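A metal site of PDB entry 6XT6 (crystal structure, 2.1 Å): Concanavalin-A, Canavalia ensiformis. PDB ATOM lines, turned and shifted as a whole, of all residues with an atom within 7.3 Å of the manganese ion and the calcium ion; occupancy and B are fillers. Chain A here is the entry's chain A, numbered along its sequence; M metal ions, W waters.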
ATOM      1  N   ALA A  89     -11.110 -26.356 -24.467  1.00  0.00           N
ATOM      2  CA  ALA A  89      -9.646 -26.382 -24.717  1.00  0.00           C
ATOM      3  C   ALA A  89      -9.356 -27.534 -25.674  1.00  0.00           C
ATOM      4  O   ALA A  89     -10.160 -28.480 -25.732  1.00  0.00           O
ATOM      5  CB  ALA A  89      -8.911 -26.542 -23.410  1.00  0.00           C
ATOM      6  N   ASP A  90      -8.247 -27.478 -26.441  1.00  0.00           N
ATOM      7  CA  ASP A  90      -7.256 -26.412 -26.457  1.00  0.00           C
ATOM      8  C   ASP A  90      -7.199 -25.668 -27.790  1.00  0.00           C
ATOM      9  O   ASP A  90      -6.666 -24.519 -27.805  1.00  0.00           O
ATOM     10  CB  ASP A  90      -5.880 -26.969 -26.136  1.00  0.00           C
ATOM     11  CG  ASP A  90      -5.746 -27.065 -24.634  1.00  0.00           C
ATOM     12  OD1 ASP A  90      -5.373 -26.035 -24.005  1.00  0.00           O
ATOM     13  OD2 ASP A  90      -6.145 -28.120 -24.101  1.00  0.00           O
ATOM     14  N   GLY A  91      -7.661 -26.315 -28.860  1.00  0.00           N
ATOM     15  CA  GLY A  91      -7.944 -25.644 -30.135  1.00  0.00           C
ATOM     16  C   GLY A  91      -7.597 -26.490 -31.346  1.00  0.00           C
ATOM     17  O   GLY A  91      -7.299 -27.691 -31.203  1.00  0.00           O
ATOM     18  N   GLY A 109      -3.128 -31.039 -25.013  1.00  0.00           N
ATOM     19  CA  GLY A 109      -3.467 -29.744 -24.392  1.00  0.00           C
ATOM     20  C   GLY A 109      -2.883 -28.575 -25.168  1.00  0.00           C
ATOM     21  O   GLY A 109      -3.065 -28.514 -26.378  1.00  0.00           O
ATOM     22  N   ARG A 110      -2.186 -27.680 -24.458  1.00  0.00           N
ATOM     23  CA  ARG A 110      -1.712 -26.339 -24.901  1.00  0.00           C
ATOM     24  C   ARG A 110      -0.757 -26.400 -26.103  1.00  0.00           C
ATOM     25  O   ARG A 110      -0.626 -25.369 -26.786  1.00  0.00           O
ATOM     26  CB  ARG A 110      -0.984 -25.675 -23.736  1.00  0.00           C
ATOM     27  CG  ARG A 110      -0.088 -26.666 -23.006  1.00  0.00           C
ATOM     28  CD  ARG A 110       1.098 -26.079 -22.300  1.00  0.00           C
ATOM     29  NE  ARG A 110       0.717 -25.419 -21.078  1.00  0.00           N
ATOM     30  CZ  ARG A 110       1.478 -25.368 -19.991  1.00  0.00           C
ATOM     31  NH1 ARG A 110       2.651 -25.964 -19.960  1.00  0.00           N
ATOM     32  NH2 ARG A 110       1.046 -24.695 -18.935  1.00  0.00           N
ATOM     33  N   LEU A 111      -0.094 -27.529 -26.382  1.00  0.00           N
ATOM     34  CA  LEU A 111       0.895 -27.653 -27.497  1.00  0.00           C
ATOM     35  C   LEU A 111       0.213 -28.100 -28.804  1.00  0.00           C
ATOM     36  O   LEU A 111       0.909 -28.160 -29.827  1.00  0.00           O
ATOM     37  CB  LEU A 111       2.019 -28.605 -27.070  1.00  0.00           C
ATOM     38  CG  LEU A 111       2.758 -28.197 -25.785  1.00  0.00           C
ATOM     39  CD1 LEU A 111       3.806 -29.216 -25.384  1.00  0.00           C
ATOM     40  CD2 LEU A 111       3.405 -26.826 -25.937  1.00  0.00           C
ATOM     41  N   LEU A 112      -1.084 -28.407 -28.775  1.00  0.00           N
ATOM     42  CA  LEU A 112      -1.963 -28.506 -29.984  1.00  0.00           C
ATOM     43  C   LEU A 112      -1.518 -29.619 -30.956  1.00  0.00           C
ATOM     44  O   LEU A 112      -1.936 -29.539 -32.134  1.00  0.00           O
ATOM     45  CB  LEU A 112      -1.967 -27.157 -30.701  1.00  0.00           C
ATOM     46  CG  LEU A 112      -2.460 -25.961 -29.902  1.00  0.00           C
ATOM     47  CD1 LEU A 112      -2.394 -24.698 -30.736  1.00  0.00           C
ATOM     48  CD2 LEU A 112      -3.870 -26.175 -29.382  1.00  0.00           C
ATOM     49  N   GLU A 142      -3.094 -21.165 -35.554  1.00  0.00           N
ATOM     50  CA  GLU A 142      -3.730 -21.797 -34.376  1.00  0.00           C
ATOM     51  C   GLU A 142      -5.055 -21.060 -34.134  1.00  0.00           C
ATOM     52  O   GLU A 142      -5.072 -19.806 -34.167  1.00  0.00           O
ATOM     53  CB  GLU A 142      -2.741 -21.832 -33.204  1.00  0.00           C
ATOM     54  CG  GLU A 142      -2.353 -20.474 -32.617  1.00  0.00           C
ATOM     55  CD  GLU A 142      -1.713 -20.507 -31.210  1.00  0.00           C
ATOM     56  OE1 GLU A 142      -0.693 -21.214 -31.001  1.00  0.00           O
ATOM     57  OE2 GLU A 142      -2.242 -19.803 -30.318  1.00  0.00           O
ATOM     58  N   LEU A 143      -6.127 -21.842 -34.024  1.00  0.00           N
ATOM     59  CA  LEU A 143      -7.432 -21.405 -33.467  1.00  0.00           C
ATOM     60  C   LEU A 143      -7.391 -21.811 -31.996  1.00  0.00           C
ATOM     61  O   LEU A 143      -7.784 -22.947 -31.692  1.00  0.00           O
ATOM     62  CB  LEU A 143      -8.588 -22.067 -34.218  1.00  0.00           C
ATOM     63  CG  LEU A 143      -9.063 -21.324 -35.461  1.00  0.00           C
ATOM     64  CD1 LEU A 143      -7.951 -21.116 -36.458  1.00  0.00           C
ATOM     65  CD2 LEU A 143     -10.237 -22.053 -36.103  1.00  0.00           C
ATOM     66  N   ASP A 144      -6.840 -20.921 -31.159  1.00  0.00           N
ATOM     67  CA  ASP A 144      -6.532 -21.210 -29.737  1.00  0.00           C
ATOM     68  C   ASP A 144      -7.719 -20.783 -28.872  1.00  0.00           C
ATOM     69  O   ASP A 144      -7.954 -19.568 -28.684  1.00  0.00           O
ATOM     70  CB  ASP A 144      -5.225 -20.540 -29.326  1.00  0.00           C
ATOM     71  CG  ASP A 144      -4.772 -21.038 -27.970  1.00  0.00           C
ATOM     72  OD1 ASP A 144      -5.619 -21.551 -27.217  1.00  0.00           O
ATOM     73  OD2 ASP A 144      -3.560 -20.932 -27.683  1.00  0.00           O
ATOM     74  N   THR A 145      -8.425 -21.773 -28.321  1.00  0.00           N
ATOM     75  CA  THR A 145      -9.708 -21.621 -27.588  1.00  0.00           C
ATOM     76  C   THR A 145      -9.475 -21.356 -26.100  1.00  0.00           C
ATOM     77  O   THR A 145     -10.435 -20.954 -25.452  1.00  0.00           O
ATOM     78  CB  THR A 145     -10.585 -22.868 -27.737  1.00  0.00           C
ATOM     79  OG1 THR A 145      -9.874 -24.018 -27.278  1.00  0.00           O
ATOM     80  CG2 THR A 145     -11.015 -23.098 -29.174  1.00  0.00           C
ATOM     81  N   TYR A 146      -8.252 -21.593 -25.598  1.00  0.00           N
ATOM     82  CA  TYR A 146      -7.921 -21.554 -24.161  1.00  0.00           C
ATOM     83  C   TYR A 146      -6.629 -20.769 -23.921  1.00  0.00           C
ATOM     84  O   TYR A 146      -5.565 -21.203 -24.322  1.00  0.00           O
ATOM     85  CB  TYR A 146      -7.793 -22.970 -23.606  1.00  0.00           C
ATOM     86  CG  TYR A 146      -7.666 -23.032 -22.108  1.00  0.00           C
ATOM     87  CD1 TYR A 146      -6.415 -22.977 -21.514  1.00  0.00           C
ATOM     88  CD2 TYR A 146      -8.779 -23.074 -21.292  1.00  0.00           C
ATOM     89  CE1 TYR A 146      -6.270 -23.042 -20.142  1.00  0.00           C
ATOM     90  CE2 TYR A 146      -8.653 -23.120 -19.908  1.00  0.00           C
ATOM     91  CZ  TYR A 146      -7.392 -23.114 -19.335  1.00  0.00           C
ATOM     92  OH  TYR A 146      -7.207 -23.148 -17.993  1.00  0.00           O
ATOM     93  N   PRO A 147      -6.714 -19.593 -23.259  1.00  0.00           N
ATOM     94  CA  PRO A 147      -5.542 -18.752 -23.020  1.00  0.00           C
ATOM     95  C   PRO A 147      -4.665 -19.339 -21.909  1.00  0.00           C
ATOM     96  O   PRO A 147      -5.109 -19.327 -20.779  1.00  0.00           O
ATOM     97  CB  PRO A 147      -6.139 -17.394 -22.636  1.00  0.00           C
ATOM     98  CG  PRO A 147      -7.456 -17.725 -21.987  1.00  0.00           C
ATOM     99  CD  PRO A 147      -7.920 -19.001 -22.667  1.00  0.00           C
ATOM    100  N   ASN A 148      -3.476 -19.836 -22.280  1.00  0.00           N
ATOM    101  CA  ASN A 148      -2.406 -20.316 -21.340  1.00  0.00           C
ATOM    102  C   ASN A 148      -1.319 -19.231 -21.228  1.00  0.00           C
ATOM    103  O   ASN A 148      -0.412 -19.209 -22.068  1.00  0.00           O
ATOM    104  CB  ASN A 148      -1.755 -21.613 -21.819  1.00  0.00           C
ATOM    105  CG  ASN A 148      -2.727 -22.707 -22.223  1.00  0.00           C
ATOM    106  OD1 ASN A 148      -3.228 -22.718 -23.358  1.00  0.00           O
ATOM    107  ND2 ASN A 148      -3.004 -23.638 -21.317  1.00  0.00           N
ATOM    108  N   THR A 149      -1.384 -18.356 -20.228  1.00  0.00           N
ATOM    109  CA  THR A 149      -0.511 -17.143 -20.174  1.00  0.00           C
ATOM    110  C   THR A 149       0.974 -17.528 -19.947  1.00  0.00           C
ATOM    111  O   THR A 149       1.819 -16.729 -20.363  1.00  0.00           O
ATOM    112  CB  THR A 149      -1.045 -16.086 -19.186  1.00  0.00           C
ATOM    113  OG1 THR A 149      -1.246 -16.705 -17.919  1.00  0.00           O
ATOM    114  CG2 THR A 149      -2.342 -15.472 -19.645  1.00  0.00           C
ATOM    115  N   ILE A 151       2.764 -19.956 -21.374  1.00  0.00           N
ATOM    116  CA  ILE A 151       3.415 -20.249 -22.677  1.00  0.00           C
ATOM    117  C   ILE A 151       3.103 -19.116 -23.652  1.00  0.00           C
ATOM    118  O   ILE A 151       3.274 -19.315 -24.857  1.00  0.00           O
ATOM    119  CB  ILE A 151       3.031 -21.643 -23.187  1.00  0.00           C
ATOM    120  CG1 ILE A 151       1.543 -21.752 -23.512  1.00  0.00           C
ATOM    121  CG2 ILE A 151       3.488 -22.696 -22.195  1.00  0.00           C
ATOM    122  CD1 ILE A 151       1.223 -22.809 -24.561  1.00  0.00           C
ATOM    123  N   GLY A 152       2.709 -17.944 -23.146  1.00  0.00           N
ATOM    124  CA  GLY A 152       2.752 -16.677 -23.895  1.00  0.00           C
ATOM    125  C   GLY A 152       1.492 -16.417 -24.705  1.00  0.00           C
ATOM    126  O   GLY A 152       1.541 -15.573 -25.592  1.00  0.00           O
ATOM    127  N   ASP A 153       0.377 -17.077 -24.390  1.00  0.00           N
ATOM    128  CA  ASP A 153      -0.936 -16.725 -24.981  1.00  0.00           C
ATOM    129  C   ASP A 153      -1.351 -15.363 -24.428  1.00  0.00           C
ATOM    130  O   ASP A 153      -1.113 -15.087 -23.254  1.00  0.00           O
ATOM    131  CB  ASP A 153      -2.000 -17.758 -24.600  1.00  0.00           C
ATOM    132  CG  ASP A 153      -1.970 -19.063 -25.389  1.00  0.00           C
ATOM    133  OD1 ASP A 153      -1.204 -19.155 -26.373  1.00  0.00           O
ATOM    134  OD2 ASP A 153      -2.741 -19.985 -25.012  1.00  0.00           O
ATOM    135  N   PRO A 154      -2.089 -14.524 -25.197  1.00  0.00           N
ATOM    136  CA  PRO A 154      -2.844 -13.434 -24.572  1.00  0.00           C
ATOM    137  C   PRO A 154      -3.990 -14.032 -23.743  1.00  0.00           C
ATOM    138  O   PRO A 154      -4.248 -15.218 -23.846  1.00  0.00           O
ATOM    139  CB  PRO A 154      -3.337 -12.622 -25.774  1.00  0.00           C
ATOM    140  CG  PRO A 154      -3.472 -13.644 -26.865  1.00  0.00           C
ATOM    141  CD  PRO A 154      -2.330 -14.620 -26.642  1.00  0.00           C
ATOM    142  N   TYR A 156      -7.166 -13.998 -23.667  1.00  0.00           N
ATOM    143  CA  TYR A 156      -8.465 -14.338 -24.318  1.00  0.00           C
ATOM    144  C   TYR A 156      -8.192 -15.404 -25.397  1.00  0.00           C
ATOM    145  O   TYR A 156      -7.043 -15.619 -25.806  1.00  0.00           O
ATOM    146  CB  TYR A 156      -9.108 -13.076 -24.907  1.00  0.00           C
ATOM    147  CG  TYR A 156      -8.104 -12.178 -25.600  1.00  0.00           C
ATOM    148  CD1 TYR A 156      -7.506 -12.561 -26.785  1.00  0.00           C
ATOM    149  CD2 TYR A 156      -7.704 -10.975 -25.039  1.00  0.00           C
ATOM    150  CE1 TYR A 156      -6.556 -11.774 -27.413  1.00  0.00           C
ATOM    151  CE2 TYR A 156      -6.746 -10.165 -25.646  1.00  0.00           C
ATOM    152  CZ  TYR A 156      -6.168 -10.564 -26.849  1.00  0.00           C
ATOM    153  OH  TYR A 156      -5.217  -9.805 -27.477  1.00  0.00           O
ATOM    154  N   HIS A 158      -7.867 -16.764 -29.131  1.00  0.00           N
ATOM    155  CA  HIS A 158      -7.131 -15.999 -30.172  1.00  0.00           C
ATOM    156  C   HIS A 158      -6.812 -16.869 -31.380  1.00  0.00           C
ATOM    157  O   HIS A 158      -6.823 -18.105 -31.278  1.00  0.00           O
ATOM    158  CB  HIS A 158      -5.866 -15.399 -29.555  1.00  0.00           C
ATOM    159  CG  HIS A 158      -5.023 -16.436 -28.870  1.00  0.00           C
ATOM    160  ND1 HIS A 158      -5.345 -16.942 -27.628  1.00  0.00           N
ATOM    161  CD2 HIS A 158      -3.905 -17.072 -29.268  1.00  0.00           C
ATOM    162  CE1 HIS A 158      -4.448 -17.829 -27.273  1.00  0.00           C
ATOM    163  NE2 HIS A 158      -3.560 -17.941 -28.251  1.00  0.00           N
ATOM    164  N   ILE A 159      -6.574 -16.222 -32.513  1.00  0.00           N
ATOM    165  CA  ILE A 159      -5.958 -16.852 -33.714  1.00  0.00           C
ATOM    166  C   ILE A 159      -4.494 -16.407 -33.691  1.00  0.00           C
ATOM    167  O   ILE A 159      -4.202 -15.280 -33.285  1.00  0.00           O
ATOM    168  CB  ILE A 159      -6.721 -16.454 -35.003  1.00  0.00           C
ATOM    169  CG1 ILE A 159      -6.556 -14.985 -35.350  1.00  0.00           C
ATOM    170  CG2 ILE A 159      -8.190 -16.809 -34.832  1.00  0.00           C
ATOM    171  CD1 ILE A 159      -7.385 -14.521 -36.559  1.00  0.00           C
ATOM    172  N   GLY A 160      -3.583 -17.277 -34.051  1.00  0.00           N
ATOM    173  CA  GLY A 160      -2.157 -16.971 -33.889  1.00  0.00           C
ATOM    174  C   GLY A 160      -1.364 -17.534 -35.022  1.00  0.00           C
ATOM    175  O   GLY A 160      -1.769 -18.617 -35.528  1.00  0.00           O
ATOM    176  N   ASP A 162       2.188 -19.135 -35.848  1.00  0.00           N
ATOM    177  CA  ASP A 162       3.263 -19.874 -35.113  1.00  0.00           C
ATOM    178  C   ASP A 162       4.353 -20.305 -36.105  1.00  0.00           C
ATOM    179  O   ASP A 162       4.043 -21.094 -37.026  1.00  0.00           O
ATOM    180  CB  ASP A 162       2.702 -21.091 -34.374  1.00  0.00           C
ATOM    181  CG  ASP A 162       1.596 -20.774 -33.376  1.00  0.00           C
ATOM    182  OD1 ASP A 162       1.374 -19.588 -33.089  1.00  0.00           O
ATOM    183  OD2 ASP A 162       0.972 -21.722 -32.897  1.00  0.00           O
ATOM    184  N   VAL A 166       5.289 -22.706 -30.491  1.00  0.00           N
ATOM    185  CA  VAL A 166       3.882 -22.523 -29.981  1.00  0.00           C
ATOM    186  C   VAL A 166       3.675 -21.062 -29.538  1.00  0.00           C
ATOM    187  O   VAL A 166       2.508 -20.601 -29.535  1.00  0.00           O
ATOM    188  CB  VAL A 166       3.585 -23.515 -28.840  1.00  0.00           C
ATOM    189  CG1 VAL A 166       4.230 -23.114 -27.528  1.00  0.00           C
ATOM    190  CG2 VAL A 166       2.090 -23.745 -28.669  1.00  0.00           C
ATOM    191  N   ARG A 167       4.749 -20.328 -29.192  1.00  0.00           N
ATOM    192  CA  ARG A 167       4.632 -18.903 -28.769  1.00  0.00           C
ATOM    193  C   ARG A 167       4.402 -18.023 -30.001  1.00  0.00           C
ATOM    194  O   ARG A 167       5.379 -17.694 -30.688  1.00  0.00           O
ATOM    195  CB  ARG A 167       5.872 -18.476 -27.993  1.00  0.00           C
ATOM    196  CG  ARG A 167       5.961 -19.105 -26.613  1.00  0.00           C
ATOM    197  CD  ARG A 167       7.343 -18.914 -26.035  1.00  0.00           C
ATOM    198  NE  ARG A 167       7.497 -19.693 -24.817  1.00  0.00           N
ATOM    199  CZ  ARG A 167       7.084 -19.325 -23.614  1.00  0.00           C
ATOM    200  NH1 ARG A 167       6.437 -18.180 -23.449  1.00  0.00           N
ATOM    201  NH2 ARG A 167       7.306 -20.111 -22.573  1.00  0.00           N
ATOM    202  N   SER A 168       3.159 -17.663 -30.281  1.00  0.00           N
ATOM    203  CA  SER A 168       2.726 -17.073 -31.565  1.00  0.00           C
ATOM    204  C   SER A 168       3.567 -15.829 -31.815  1.00  0.00           C
ATOM    205  O   SER A 168       3.881 -15.155 -30.847  1.00  0.00           O
ATOM    206  CB  SER A 168       1.257 -16.767 -31.568  1.00  0.00           C
ATOM    207  OG  SER A 168       0.510 -17.907 -31.148  1.00  0.00           O
ATOM    208  N   THR A 171      -0.829 -12.502 -32.828  1.00  0.00           N
ATOM    209  CA  THR A 171      -2.162 -13.057 -32.462  1.00  0.00           C
ATOM    210  C   THR A 171      -3.222 -11.991 -32.704  1.00  0.00           C
ATOM    211  O   THR A 171      -2.850 -10.824 -32.767  1.00  0.00           O
ATOM    212  CB  THR A 171      -2.189 -13.496 -30.995  1.00  0.00           C
ATOM    213  OG1 THR A 171      -2.000 -12.267 -30.306  1.00  0.00           O
ATOM    214  CG2 THR A 171      -1.111 -14.485 -30.632  1.00  0.00           C
HETATM  215 MN    MN M   1      -2.053 -19.482 -28.402  1.00  0.00          MN
HETATM  216 CA    CA M   2      -3.727 -21.978 -25.551  1.00  0.00          CA
HETATM  217  O   HOH W   1      -1.830 -22.786 -26.659  1.00  0.00           O
HETATM  218  O   HOH W   2      -0.577 -20.943 -28.406  1.00  0.00           O
HETATM  219  O   HOH W   3      -0.671 -18.200 -28.860  1.00  0.00           O
HETATM  220  O   HOH W   4      -4.825 -24.088 -25.930  1.00  0.00           O
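The side-chain carboxylate of Glu 142 lies close to the side-chain hydroxyl of Ser 168, 3.4 Å away.
OE1 of Glu 142 lies close to OD2 of Asp 162, 2.6 Å away.
The backbone NH (N) of Glu 142 lies within hydrogen-bond range of the backbone carbonyl oxygen (O) of Gly 160, 2.9 Å away.
A ring nitrogen (ND1) of His 158 lies within hydrogen-bond range of the backbone carbonyl oxygen of Tyr 156 (2.8 Å).
The calcium ion is bound by OD2 of Asp 153, at 2.3 Å.
The calcium ion is bound by water W1 (2.3 Å).
O of Tyr 146 binds the calcium ion.
OD1 of Asn 148 binds the calcium ion (2.4 Å).
The calcium ion is bound by OD2 of Asp 144 (2.4 Å).
Water W4 binds the calcium ion, 2.4 Å away.
OD1 of Asp 144 is bound to the calcium ion, 2.6 Å away.
The calcium ion has seven donor atoms within binding distance.
Four residues have an atom within 4 Å of the calcium ion: Asp 144, Tyr 146, Asn 148 and Asp 153.
Within 4 Å of the manganese ion: Glu 142, Asp 144, Asp 153 and His 158.
Water W2 bridges OE1 of Glu 142 and O of Val 166.
Water W3 binds the manganese ion, 1.9 Å away.
OE2 of Glu 142 is bound to the manganese ion.
Water W2 binds the manganese ion (2.1 Å).
The manganese ion is bound by a ring nitrogen (NE2) of His 158.
OD2 of Asp 144 is bound to the manganese ion (2.2 Å).
The manganese ion is bound by the side-chain carboxylate (OD1) of Asp 153, 2.2 Å away.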
